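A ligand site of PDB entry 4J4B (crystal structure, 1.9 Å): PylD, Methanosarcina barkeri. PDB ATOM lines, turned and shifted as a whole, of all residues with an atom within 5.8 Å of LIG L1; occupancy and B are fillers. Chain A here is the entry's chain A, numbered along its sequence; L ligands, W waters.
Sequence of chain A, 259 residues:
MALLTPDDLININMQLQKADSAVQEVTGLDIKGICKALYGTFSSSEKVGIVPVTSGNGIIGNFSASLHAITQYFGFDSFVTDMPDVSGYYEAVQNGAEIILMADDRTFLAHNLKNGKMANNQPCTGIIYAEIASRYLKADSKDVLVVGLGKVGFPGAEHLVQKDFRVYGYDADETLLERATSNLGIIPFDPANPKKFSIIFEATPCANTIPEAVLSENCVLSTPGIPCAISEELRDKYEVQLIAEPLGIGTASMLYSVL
Leu 3 touches LIG L1 (CA to O1, 3.7 Å).
Pro 52 touches LIG L1 (CA to O3, 3.5 Å).
O of Gly 58 touches C10 of LIG L1, at 3.4 Å.
Ile 59 touches LIG L1 (CA to O2, 3.6 Å).
Phe 63 touches LIG L1.
O of Asp 104 touches C6 of LIG L1, at 3.7 Å.
OD1 of Asn 121 touches C3 of LIG L1, 3.6 Å away.
O of Pro 246 touches N1 of LIG L1, 3.6 Å away.
CD1 of Leu 247 touches C5 of LIG L1 (3.6 Å).
Hydrophobic or aromatic side chains that line LIG L1: Leu 3, Leu 4, Val 53, Ile 59, Ile 60, Phe 63 and Leu 247.
An oxygen (O3) of LIG L1 is in hydrogen-bond range of the backbone NH (N) of Val 53, 2.8 Å away.
The backbone carbonyl oxygen (O) of Val 53 lies within hydrogen-bond range of a nitrogen (N4) of LIG L1 (2.7 Å).
The backbone NH (N) of Ile 60 is in hydrogen-bond range of an oxygen (O2) of LIG L1, 3.0 Å away.
The backbone carbonyl oxygen of Pro 246 is in hydrogen-bond range of a nitrogen (N7) of LG2 L2, 3.3 Å away.
The backbone carbonyl oxygen (O) of Ala 103 sits at hydrogen-bond distance from a nitrogen (N4) of LIG L1, 2.9 Å away.
An oxygen (O1) of LIG L1 lies within hydrogen-bond range of the backbone NH (N) of Leu 4 (3.1 Å).
The backbone carbonyl oxygen of Ala 2 is in hydrogen-bond range of an oxygen (O13) of LG2 L2, at 2.9 Å.
The backbone carbonyl oxygen (O) of Phe 108 lies within hydrogen-bond range of the backbone NH (N) of Asn 121 (2.8 Å).
The backbone NH (N) of Ile 59 sits at hydrogen-bond distance from the backbone carbonyl oxygen (O) of Val 53, at 3.5 Å.
Water W1 lies within hydrogen-bond range of N3 of LIG L1 (2.8 Å), O of Asp 104 (2.9 Å) and N of Phe 108 (3.5 Å).
Water W2 lies within hydrogen-bond range of an oxygen (O2) of LIG L1 (2.8 Å), the backbone NH of Ser 64 (3.1 Å) and the backbone carbonyl oxygen of Ile 60 (3.3 Å).
Water W5 lies within hydrogen-bond range of O of Ser 55 (2.6 Å), OD1 of Asp 105 (2.8 Å) and N4 of LIG L1 (2.8 Å).
Water W4 lies within hydrogen-bond range of O of Val 51, N of Ala 103 and O3 of LIG L1.
Water W3 lies within hydrogen-bond range of O of Pro 246 (2.8 Å), N1 of LIG L1 (3.2 Å) and N7 of LG2 L2 (3.4 Å).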
ATOM      1  N   ALA A   2     -28.303  -0.042 -29.154  1.00  0.00           N
ATOM      2  CA  ALA A   2     -27.978  -1.049 -30.157  1.00  0.00           C
ATOM      3  C   ALA A   2     -27.150  -2.188 -29.562  1.00  0.00           C
ATOM      4  O   ALA A   2     -25.918  -2.207 -29.653  1.00  0.00           O
ATOM      5  CB  ALA A   2     -27.237  -0.397 -31.323  1.00  0.00           C
ATOM      6  N   LEU A   3     -27.856  -3.131 -28.930  1.00  0.00           N
ATOM      7  CA  LEU A   3     -27.226  -4.259 -28.246  1.00  0.00           C
ATOM      8  C   LEU A   3     -27.217  -5.510 -29.131  1.00  0.00           C
ATOM      9  O   LEU A   3     -27.981  -5.600 -30.093  1.00  0.00           O
ATOM     10  CB  LEU A   3     -27.965  -4.576 -26.936  1.00  0.00           C
ATOM     11  CG  LEU A   3     -28.093  -3.522 -25.836  1.00  0.00           C
ATOM     12  CD1 LEU A   3     -28.866  -4.110 -24.655  1.00  0.00           C
ATOM     13  CD2 LEU A   3     -26.743  -2.991 -25.377  1.00  0.00           C
ATOM     14  N   LEU A   4     -26.342  -6.456 -28.803  1.00  0.00           N
ATOM     15  CA  LEU A   4     -26.319  -7.748 -29.474  1.00  0.00           C
ATOM     16  C   LEU A   4     -27.610  -8.531 -29.219  1.00  0.00           C
ATOM     17  O   LEU A   4     -28.149  -8.512 -28.112  1.00  0.00           O
ATOM     18  CB  LEU A   4     -25.120  -8.587 -29.017  1.00  0.00           C
ATOM     19  CG  LEU A   4     -23.725  -8.307 -29.578  1.00  0.00           C
ATOM     20  CD1 LEU A   4     -22.682  -9.070 -28.779  1.00  0.00           C
ATOM     21  CD2 LEU A   4     -23.636  -8.667 -31.056  1.00  0.00           C
ATOM     22  N   VAL A  51     -18.304 -13.505 -16.597  1.00  0.00           N
ATOM     23  CA  VAL A  51     -19.369 -13.361 -15.606  1.00  0.00           C
ATOM     24  C   VAL A  51     -20.639 -12.854 -16.280  1.00  0.00           C
ATOM     25  O   VAL A  51     -20.696 -11.698 -16.690  1.00  0.00           O
ATOM     26  CB  VAL A  51     -18.961 -12.430 -14.450  1.00  0.00           C
ATOM     27  CG1 VAL A  51     -20.100 -12.290 -13.439  1.00  0.00           C
ATOM     28  CG2 VAL A  51     -17.705 -12.943 -13.756  1.00  0.00           C
ATOM     29  N   PRO A  52     -21.667 -13.731 -16.388  1.00  0.00           N
ATOM     30  CA  PRO A  52     -22.966 -13.299 -16.893  1.00  0.00           C
ATOM     31  C   PRO A  52     -23.551 -12.243 -15.970  1.00  0.00           C
ATOM     32  O   PRO A  52     -23.369 -12.296 -14.754  1.00  0.00           O
ATOM     33  CB  PRO A  52     -23.806 -14.582 -16.826  1.00  0.00           C
ATOM     34  CG  PRO A  52     -22.795 -15.684 -16.903  1.00  0.00           C
ATOM     35  CD  PRO A  52     -21.643 -15.177 -16.104  1.00  0.00           C
ATOM     36  N   VAL A  53     -24.229 -11.263 -16.568  1.00  0.00           N
ATOM     37  CA  VAL A  53     -24.801 -10.134 -15.840  1.00  0.00           C
ATOM     38  C   VAL A  53     -26.277  -9.950 -16.213  1.00  0.00           C
ATOM     39  O   VAL A  53     -26.618  -9.824 -17.384  1.00  0.00           O
ATOM     40  CB  VAL A  53     -23.981  -8.836 -16.086  1.00  0.00           C
ATOM     41  CG1 VAL A  53     -24.696  -7.615 -15.528  1.00  0.00           C
ATOM     42  CG2 VAL A  53     -22.595  -8.951 -15.472  1.00  0.00           C
ATOM     43  N   THR A  54     -27.128  -9.950 -15.184  1.00  0.00           N
ATOM     44  CA  THR A  54     -28.586  -9.840 -15.369  1.00  0.00           C
ATOM     45  C   THR A  54     -29.080  -8.389 -15.322  1.00  0.00           C
ATOM     46  O   THR A  54     -30.274  -8.127 -15.435  1.00  0.00           O
ATOM     47  CB  THR A  54     -29.345 -10.635 -14.287  1.00  0.00           C
ATOM     48  OG1 THR A  54     -29.045 -10.105 -12.996  1.00  0.00           O
ATOM     49  CG2 THR A  54     -28.972 -12.102 -14.332  1.00  0.00           C
ATOM     50  N   SER A  55     -28.152  -7.450 -15.157  1.00  0.00           N
ATOM     51  CA  SER A  55     -28.459  -6.011 -15.078  1.00  0.00           C
ATOM     52  C   SER A  55     -29.143  -5.491 -16.345  1.00  0.00           C
ATOM     53  O   SER A  55     -28.928  -6.022 -17.438  1.00  0.00           O
ATOM     54  CB  SER A  55     -27.174  -5.222 -14.812  1.00  0.00           C
ATOM     55  OG  SER A  55     -27.365  -3.830 -14.951  1.00  0.00           O
ATOM     56  N   GLY A  58     -30.682  -7.496 -19.204  1.00  0.00           N
ATOM     57  CA  GLY A  58     -30.333  -8.807 -18.671  1.00  0.00           C
ATOM     58  C   GLY A  58     -29.399  -9.626 -19.541  1.00  0.00           C
ATOM     59  O   GLY A  58     -28.736  -9.104 -20.434  1.00  0.00           O
ATOM     60  N   ILE A  59     -29.356 -10.918 -19.236  1.00  0.00           N
ATOM     61  CA  ILE A  59     -28.510 -11.863 -19.948  1.00  0.00           C
ATOM     62  C   ILE A  59     -28.937 -11.969 -21.416  1.00  0.00           C
ATOM     63  O   ILE A  59     -30.125 -12.089 -21.716  1.00  0.00           O
ATOM     64  CB  ILE A  59     -28.523 -13.259 -19.257  1.00  0.00           C
ATOM     65  CG1 ILE A  59     -27.839 -13.166 -17.878  1.00  0.00           C
ATOM     66  CG2 ILE A  59     -27.846 -14.310 -20.124  1.00  0.00           C
ATOM     67  CD1 ILE A  59     -27.978 -14.402 -17.027  1.00  0.00           C
ATOM     68  N   ILE A  60     -27.964 -11.864 -22.317  1.00  0.00           N
ATOM     69  CA  ILE A  60     -28.208 -12.060 -23.731  1.00  0.00           C
ATOM     70  C   ILE A  60     -27.822 -13.483 -24.098  1.00  0.00           C
ATOM     71  O   ILE A  60     -26.709 -13.929 -23.817  1.00  0.00           O
ATOM     72  CB  ILE A  60     -27.430 -11.033 -24.600  1.00  0.00           C
ATOM     73  CG1 ILE A  60     -27.908  -9.604 -24.290  1.00  0.00           C
ATOM     74  CG2 ILE A  60     -27.602 -11.333 -26.089  1.00  0.00           C
ATOM     75  CD1 ILE A  60     -27.088  -8.514 -24.925  1.00  0.00           C
ATOM     76  N   GLY A  61     -28.766 -14.211 -24.696  1.00  0.00           N
ATOM     77  CA  GLY A  61     -28.530 -15.588 -25.135  1.00  0.00           C
ATOM     78  C   GLY A  61     -27.350 -15.659 -26.078  1.00  0.00           C
ATOM     79  O   GLY A  61     -27.227 -14.836 -26.992  1.00  0.00           O
ATOM     80  N   PHE A  63     -24.320 -14.895 -25.522  1.00  0.00           N
ATOM     81  CA  PHE A  63     -23.271 -13.901 -25.223  1.00  0.00           C
ATOM     82  C   PHE A  63     -22.065 -14.475 -24.477  1.00  0.00           C
ATOM     83  O   PHE A  63     -20.945 -14.430 -24.986  1.00  0.00           O
ATOM     84  CB  PHE A  63     -23.844 -12.679 -24.478  1.00  0.00           C
ATOM     85  CG  PHE A  63     -22.830 -11.584 -24.262  1.00  0.00           C
ATOM     86  CD1 PHE A  63     -22.482 -10.727 -25.308  1.00  0.00           C
ATOM     87  CD2 PHE A  63     -22.233 -11.396 -23.024  1.00  0.00           C
ATOM     88  CE1 PHE A  63     -21.548  -9.723 -25.112  1.00  0.00           C
ATOM     89  CE2 PHE A  63     -21.299 -10.392 -22.828  1.00  0.00           C
ATOM     90  CZ  PHE A  63     -20.961  -9.556 -23.872  1.00  0.00           C
ATOM     91  N   SER A  64     -22.302 -15.010 -23.277  1.00  0.00           N
ATOM     92  CA  SER A  64     -21.228 -15.581 -22.471  1.00  0.00           C
ATOM     93  C   SER A  64     -20.609 -16.812 -23.125  1.00  0.00           C
ATOM     94  O   SER A  64     -19.411 -17.068 -22.972  1.00  0.00           O
ATOM     95  CB  SER A  64     -21.711 -15.903 -21.057  1.00  0.00           C
ATOM     96  OG  SER A  64     -22.590 -17.011 -21.044  1.00  0.00           O
ATOM     97  N   ALA A 103     -20.091  -7.615 -18.705  1.00  0.00           N
ATOM     98  CA  ALA A 103     -20.772  -6.516 -19.394  1.00  0.00           C
ATOM     99  C   ALA A 103     -22.190  -6.258 -18.897  1.00  0.00           C
ATOM    100  O   ALA A 103     -22.985  -7.199 -18.763  1.00  0.00           O
ATOM    101  CB  ALA A 103     -20.810  -6.803 -20.893  1.00  0.00           C
ATOM    102  N   ASP A 104     -22.499  -4.986 -18.639  1.00  0.00           N
ATOM    103  CA  ASP A 104     -23.894  -4.557 -18.564  1.00  0.00           C
ATOM    104  C   ASP A 104     -24.286  -3.851 -19.863  1.00  0.00           C
ATOM    105  O   ASP A 104     -23.565  -3.952 -20.856  1.00  0.00           O
ATOM    106  CB  ASP A 104     -24.220  -3.761 -17.273  1.00  0.00           C
ATOM    107  CG  ASP A 104     -23.488  -2.419 -17.171  1.00  0.00           C
ATOM    108  OD1 ASP A 104     -23.045  -1.857 -18.198  1.00  0.00           O
ATOM    109  OD2 ASP A 104     -23.377  -1.924 -16.029  1.00  0.00           O
ATOM    110  N   ASP A 105     -25.430  -3.153 -19.880  1.00  0.00           N
ATOM    111  CA  ASP A 105     -25.936  -2.544 -21.111  1.00  0.00           C
ATOM    112  C   ASP A 105     -25.107  -1.353 -21.606  1.00  0.00           C
ATOM    113  O   ASP A 105     -25.128  -1.029 -22.795  1.00  0.00           O
ATOM    114  CB  ASP A 105     -27.406  -2.131 -20.954  1.00  0.00           C
ATOM    115  CG  ASP A 105     -28.347  -3.321 -20.826  1.00  0.00           C
ATOM    116  OD1 ASP A 105     -27.869  -4.469 -20.809  1.00  0.00           O
ATOM    117  OD2 ASP A 105     -29.584  -3.100 -20.745  1.00  0.00           O
ATOM    118  N   PHE A 108     -18.981  -2.778 -21.315  1.00  0.00           N
ATOM    119  CA  PHE A 108     -18.368  -4.106 -21.454  1.00  0.00           C
ATOM    120  C   PHE A 108     -16.869  -3.953 -21.190  1.00  0.00           C
ATOM    121  O   PHE A 108     -16.164  -3.282 -21.954  1.00  0.00           O
ATOM    122  CB  PHE A 108     -18.672  -4.690 -22.840  1.00  0.00           C
ATOM    123  CG  PHE A 108     -17.983  -6.012 -23.131  1.00  0.00           C
ATOM    124  CD1 PHE A 108     -17.727  -6.938 -22.129  1.00  0.00           C
ATOM    125  CD2 PHE A 108     -17.638  -6.327 -24.440  1.00  0.00           C
ATOM    126  CE1 PHE A 108     -17.108  -8.146 -22.418  1.00  0.00           C
ATOM    127  CE2 PHE A 108     -17.019  -7.535 -24.729  1.00  0.00           C
ATOM    128  CZ  PHE A 108     -16.753  -8.440 -23.719  1.00  0.00           C
ATOM    129  N   ASN A 121     -14.717  -1.857 -23.951  1.00  0.00           N
ATOM    130  CA  ASN A 121     -15.032  -2.401 -25.273  1.00  0.00           C
ATOM    131  C   ASN A 121     -15.124  -1.368 -26.397  1.00  0.00           C
ATOM    132  O   ASN A 121     -14.669  -1.616 -27.504  1.00  0.00           O
ATOM    133  CB  ASN A 121     -16.330  -3.202 -25.211  1.00  0.00           C
ATOM    134  CG  ASN A 121     -16.703  -3.808 -26.554  1.00  0.00           C
ATOM    135  OD1 ASN A 121     -17.739  -3.467 -27.124  1.00  0.00           O
ATOM    136  ND2 ASN A 121     -15.862  -4.712 -27.057  1.00  0.00           N
ATOM    137  N   PRO A 246     -19.250  -9.535 -35.122  1.00  0.00           N
ATOM    138  CA  PRO A 246     -20.102  -9.002 -34.041  1.00  0.00           C
ATOM    139  C   PRO A 246     -19.492  -8.841 -32.633  1.00  0.00           C
ATOM    140  O   PRO A 246     -20.040  -8.077 -31.835  1.00  0.00           O
ATOM    141  CB  PRO A 246     -21.243 -10.020 -33.972  1.00  0.00           C
ATOM    142  CG  PRO A 246     -20.626 -11.294 -34.436  1.00  0.00           C
ATOM    143  CD  PRO A 246     -19.706 -10.873 -35.537  1.00  0.00           C
ATOM    144  N   LEU A 247     -18.399  -9.545 -32.316  1.00  0.00           N
ATOM    145  CA  LEU A 247     -17.899  -9.545 -30.933  1.00  0.00           C
ATOM    146  C   LEU A 247     -16.399  -9.842 -30.775  1.00  0.00           C
ATOM    147  O   LEU A 247     -15.709  -9.178 -29.993  1.00  0.00           O
ATOM    148  CB  LEU A 247     -18.725 -10.511 -30.072  1.00  0.00           C
ATOM    149  CG  LEU A 247     -18.493 -10.644 -28.559  1.00  0.00           C
ATOM    150  CD1 LEU A 247     -18.583  -9.313 -27.843  1.00  0.00           C
ATOM    151  CD2 LEU A 247     -19.466 -11.654 -27.971  1.00  0.00           C
HETATM  152  O1  LIG L   1     -24.181  -5.734 -26.743  1.00  0.00           O
HETATM  153  C1  LIG L   1     -23.441  -5.070 -26.015  1.00  0.00           C
HETATM  154  C2  LIG L   1     -22.319  -4.257 -26.599  1.00  0.00           C
HETATM  155  C3  LIG L   1     -20.986  -4.983 -26.444  1.00  0.00           C
HETATM  156  C4  LIG L   1     -20.926  -6.292 -27.220  1.00  0.00           C
HETATM  157  C5  LIG L   1     -20.167  -6.127 -28.534  1.00  0.00           C
HETATM  158  N1  LIG L   1     -21.027  -5.500 -29.529  1.00  0.00           N
HETATM  159  N2  LIG L   1     -22.580  -3.954 -27.989  1.00  0.00           N
HETATM  160  N3  LIG L   1     -23.559  -5.026 -24.699  1.00  0.00           N
HETATM  161  C6  LIG L   1     -24.553  -5.761 -23.962  1.00  0.00           C
HETATM  162  C7  LIG L   1     -23.964  -7.019 -23.347  1.00  0.00           C
HETATM  163  C8  LIG L   1     -24.789  -7.449 -22.136  1.00  0.00           C
HETATM  164  C9  LIG L   1     -24.346  -8.837 -21.689  1.00  0.00           C
HETATM  165  C10 LIG L   1     -25.320  -9.455 -20.700  1.00  0.00           C
HETATM  166  N4  LIG L   1     -25.359  -8.660 -19.485  1.00  0.00           N
HETATM  167  C11 LIG L   1     -24.854 -10.853 -20.391  1.00  0.00           C
HETATM  168  O2  LIG L   1     -25.170 -11.766 -21.186  1.00  0.00           O
HETATM  169  O3  LIG L   1     -24.176 -11.074 -19.365  1.00  0.00           O
HETATM  170  P1  LG2 L   2     -23.056   5.347 -30.501  1.00  0.00           P
HETATM  171  O1  LG2 L   2     -24.541   5.655 -30.505  1.00  0.00           O
HETATM  172  O2  LG2 L   2     -22.195   5.834 -29.358  1.00  0.00           O
HETATM  173  O3  LG2 L   2     -22.405   5.872 -31.867  1.00  0.00           O
HETATM  174  C1  LG2 L   2     -23.104   5.759 -33.103  1.00  0.00           C
HETATM  175  C2  LG2 L   2     -22.988   7.080 -33.868  1.00  0.00           C
HETATM  176  O4  LG2 L   2     -23.383   6.898 -35.227  1.00  0.00           O
HETATM  177  C3  LG2 L   2     -23.893   8.161 -33.278  1.00  0.00           C
HETATM  178  O5  LG2 L   2     -23.093   9.314 -32.994  1.00  0.00           O
HETATM  179  C4  LG2 L   2     -24.892   8.485 -34.373  1.00  0.00           C
HETATM  180  O6  LG2 L   2     -25.158   9.893 -34.425  1.00  0.00           O
HETATM  181  C5  LG2 L   2     -24.192   8.012 -35.631  1.00  0.00           C
HETATM  182  N1  LG2 L   2     -25.143   7.638 -36.714  1.00  0.00           N
HETATM  183  C6  LG2 L   2     -26.277   6.920 -36.597  1.00  0.00           C
HETATM  184  N2  LG2 L   2     -26.891   6.770 -37.793  1.00  0.00           N
HETATM  185  C7  LG2 L   2     -26.151   7.417 -38.712  1.00  0.00           C
HETATM  186  C8  LG2 L   2     -26.219   7.653 -40.172  1.00  0.00           C
HETATM  187  N3  LG2 L   2     -27.249   7.160 -40.913  1.00  0.00           N
HETATM  188  N4  LG2 L   2     -25.232   8.371 -40.744  1.00  0.00           N
HETATM  189  C9  LG2 L   2     -24.199   8.871 -40.025  1.00  0.00           C
HETATM  190  N5  LG2 L   2     -24.078   8.695 -38.698  1.00  0.00           N
HETATM  191  C10 LG2 L   2     -24.994   7.982 -38.002  1.00  0.00           C
HETATM  192  O7  LG2 L   2     -22.906   3.746 -30.623  1.00  0.00           O
HETATM  193  P2  LG2 L   2     -21.458   3.053 -30.485  1.00  0.00           P
HETATM  194  O8  LG2 L   2     -21.278   2.649 -29.042  1.00  0.00           O
HETATM  195  O9  LG2 L   2     -20.416   3.931 -31.133  1.00  0.00           O
HETATM  196  O10 LG2 L   2     -21.623   1.717 -31.376  1.00  0.00           O
HETATM  197  C11 LG2 L   2     -21.749   1.788 -32.801  1.00  0.00           C
HETATM  198  C12 LG2 L   2     -22.153   0.418 -33.356  1.00  0.00           C
HETATM  199  O11 LG2 L   2     -21.117  -0.541 -33.143  1.00  0.00           O
HETATM  200  C13 LG2 L   2     -23.397  -0.135 -32.688  1.00  0.00           C
HETATM  201  O12 LG2 L   2     -24.205  -0.701 -33.729  1.00  0.00           O
HETATM  202  C14 LG2 L   2     -22.901  -1.259 -31.801  1.00  0.00           C
HETATM  203  O13 LG2 L   2     -23.885  -2.290 -31.704  1.00  0.00           O
HETATM  204  C15 LG2 L   2     -21.659  -1.727 -32.541  1.00  0.00           C
HETATM  205  N6  LG2 L   2     -20.615  -2.390 -31.746  1.00  0.00           N
HETATM  206  C16 LG2 L   2     -19.995  -3.428 -32.327  1.00  0.00           C
HETATM  207  C17 LG2 L   2     -18.974  -4.145 -31.702  1.00  0.00           C
HETATM  208  C18 LG2 L   2     -18.342  -5.306 -32.427  1.00  0.00           C
HETATM  209  O14 LG2 L   2     -17.420  -5.915 -31.926  1.00  0.00           O
HETATM  210  N7  LG2 L   2     -18.793  -5.636 -33.639  1.00  0.00           N
HETATM  211  C19 LG2 L   2     -18.510  -3.739 -30.314  1.00  0.00           C
HETATM  212  C20 LG2 L   2     -19.258  -2.584 -29.803  1.00  0.00           C
HETATM  213  C21 LG2 L   2     -20.264  -1.953 -30.525  1.00  0.00           C
HETATM  214  O   HOH W   1     -21.818  -3.492 -23.149  1.00  0.00           O
HETATM  215  O   HOH W   2     -24.677 -14.527 -21.271  1.00  0.00           O
HETATM  216  O   HOH W   3     -21.962  -6.167 -32.553  1.00  0.00           O
HETATM  217  O   HOH W   4     -21.404 -10.200 -18.888  1.00  0.00           O
HETATM  218  O   HOH W   5     -26.855  -6.299 -19.012  1.00  0.00           O
HETATM  219  O   HOH W   6     -19.908  -1.668 -26.308  1.00  0.00           O
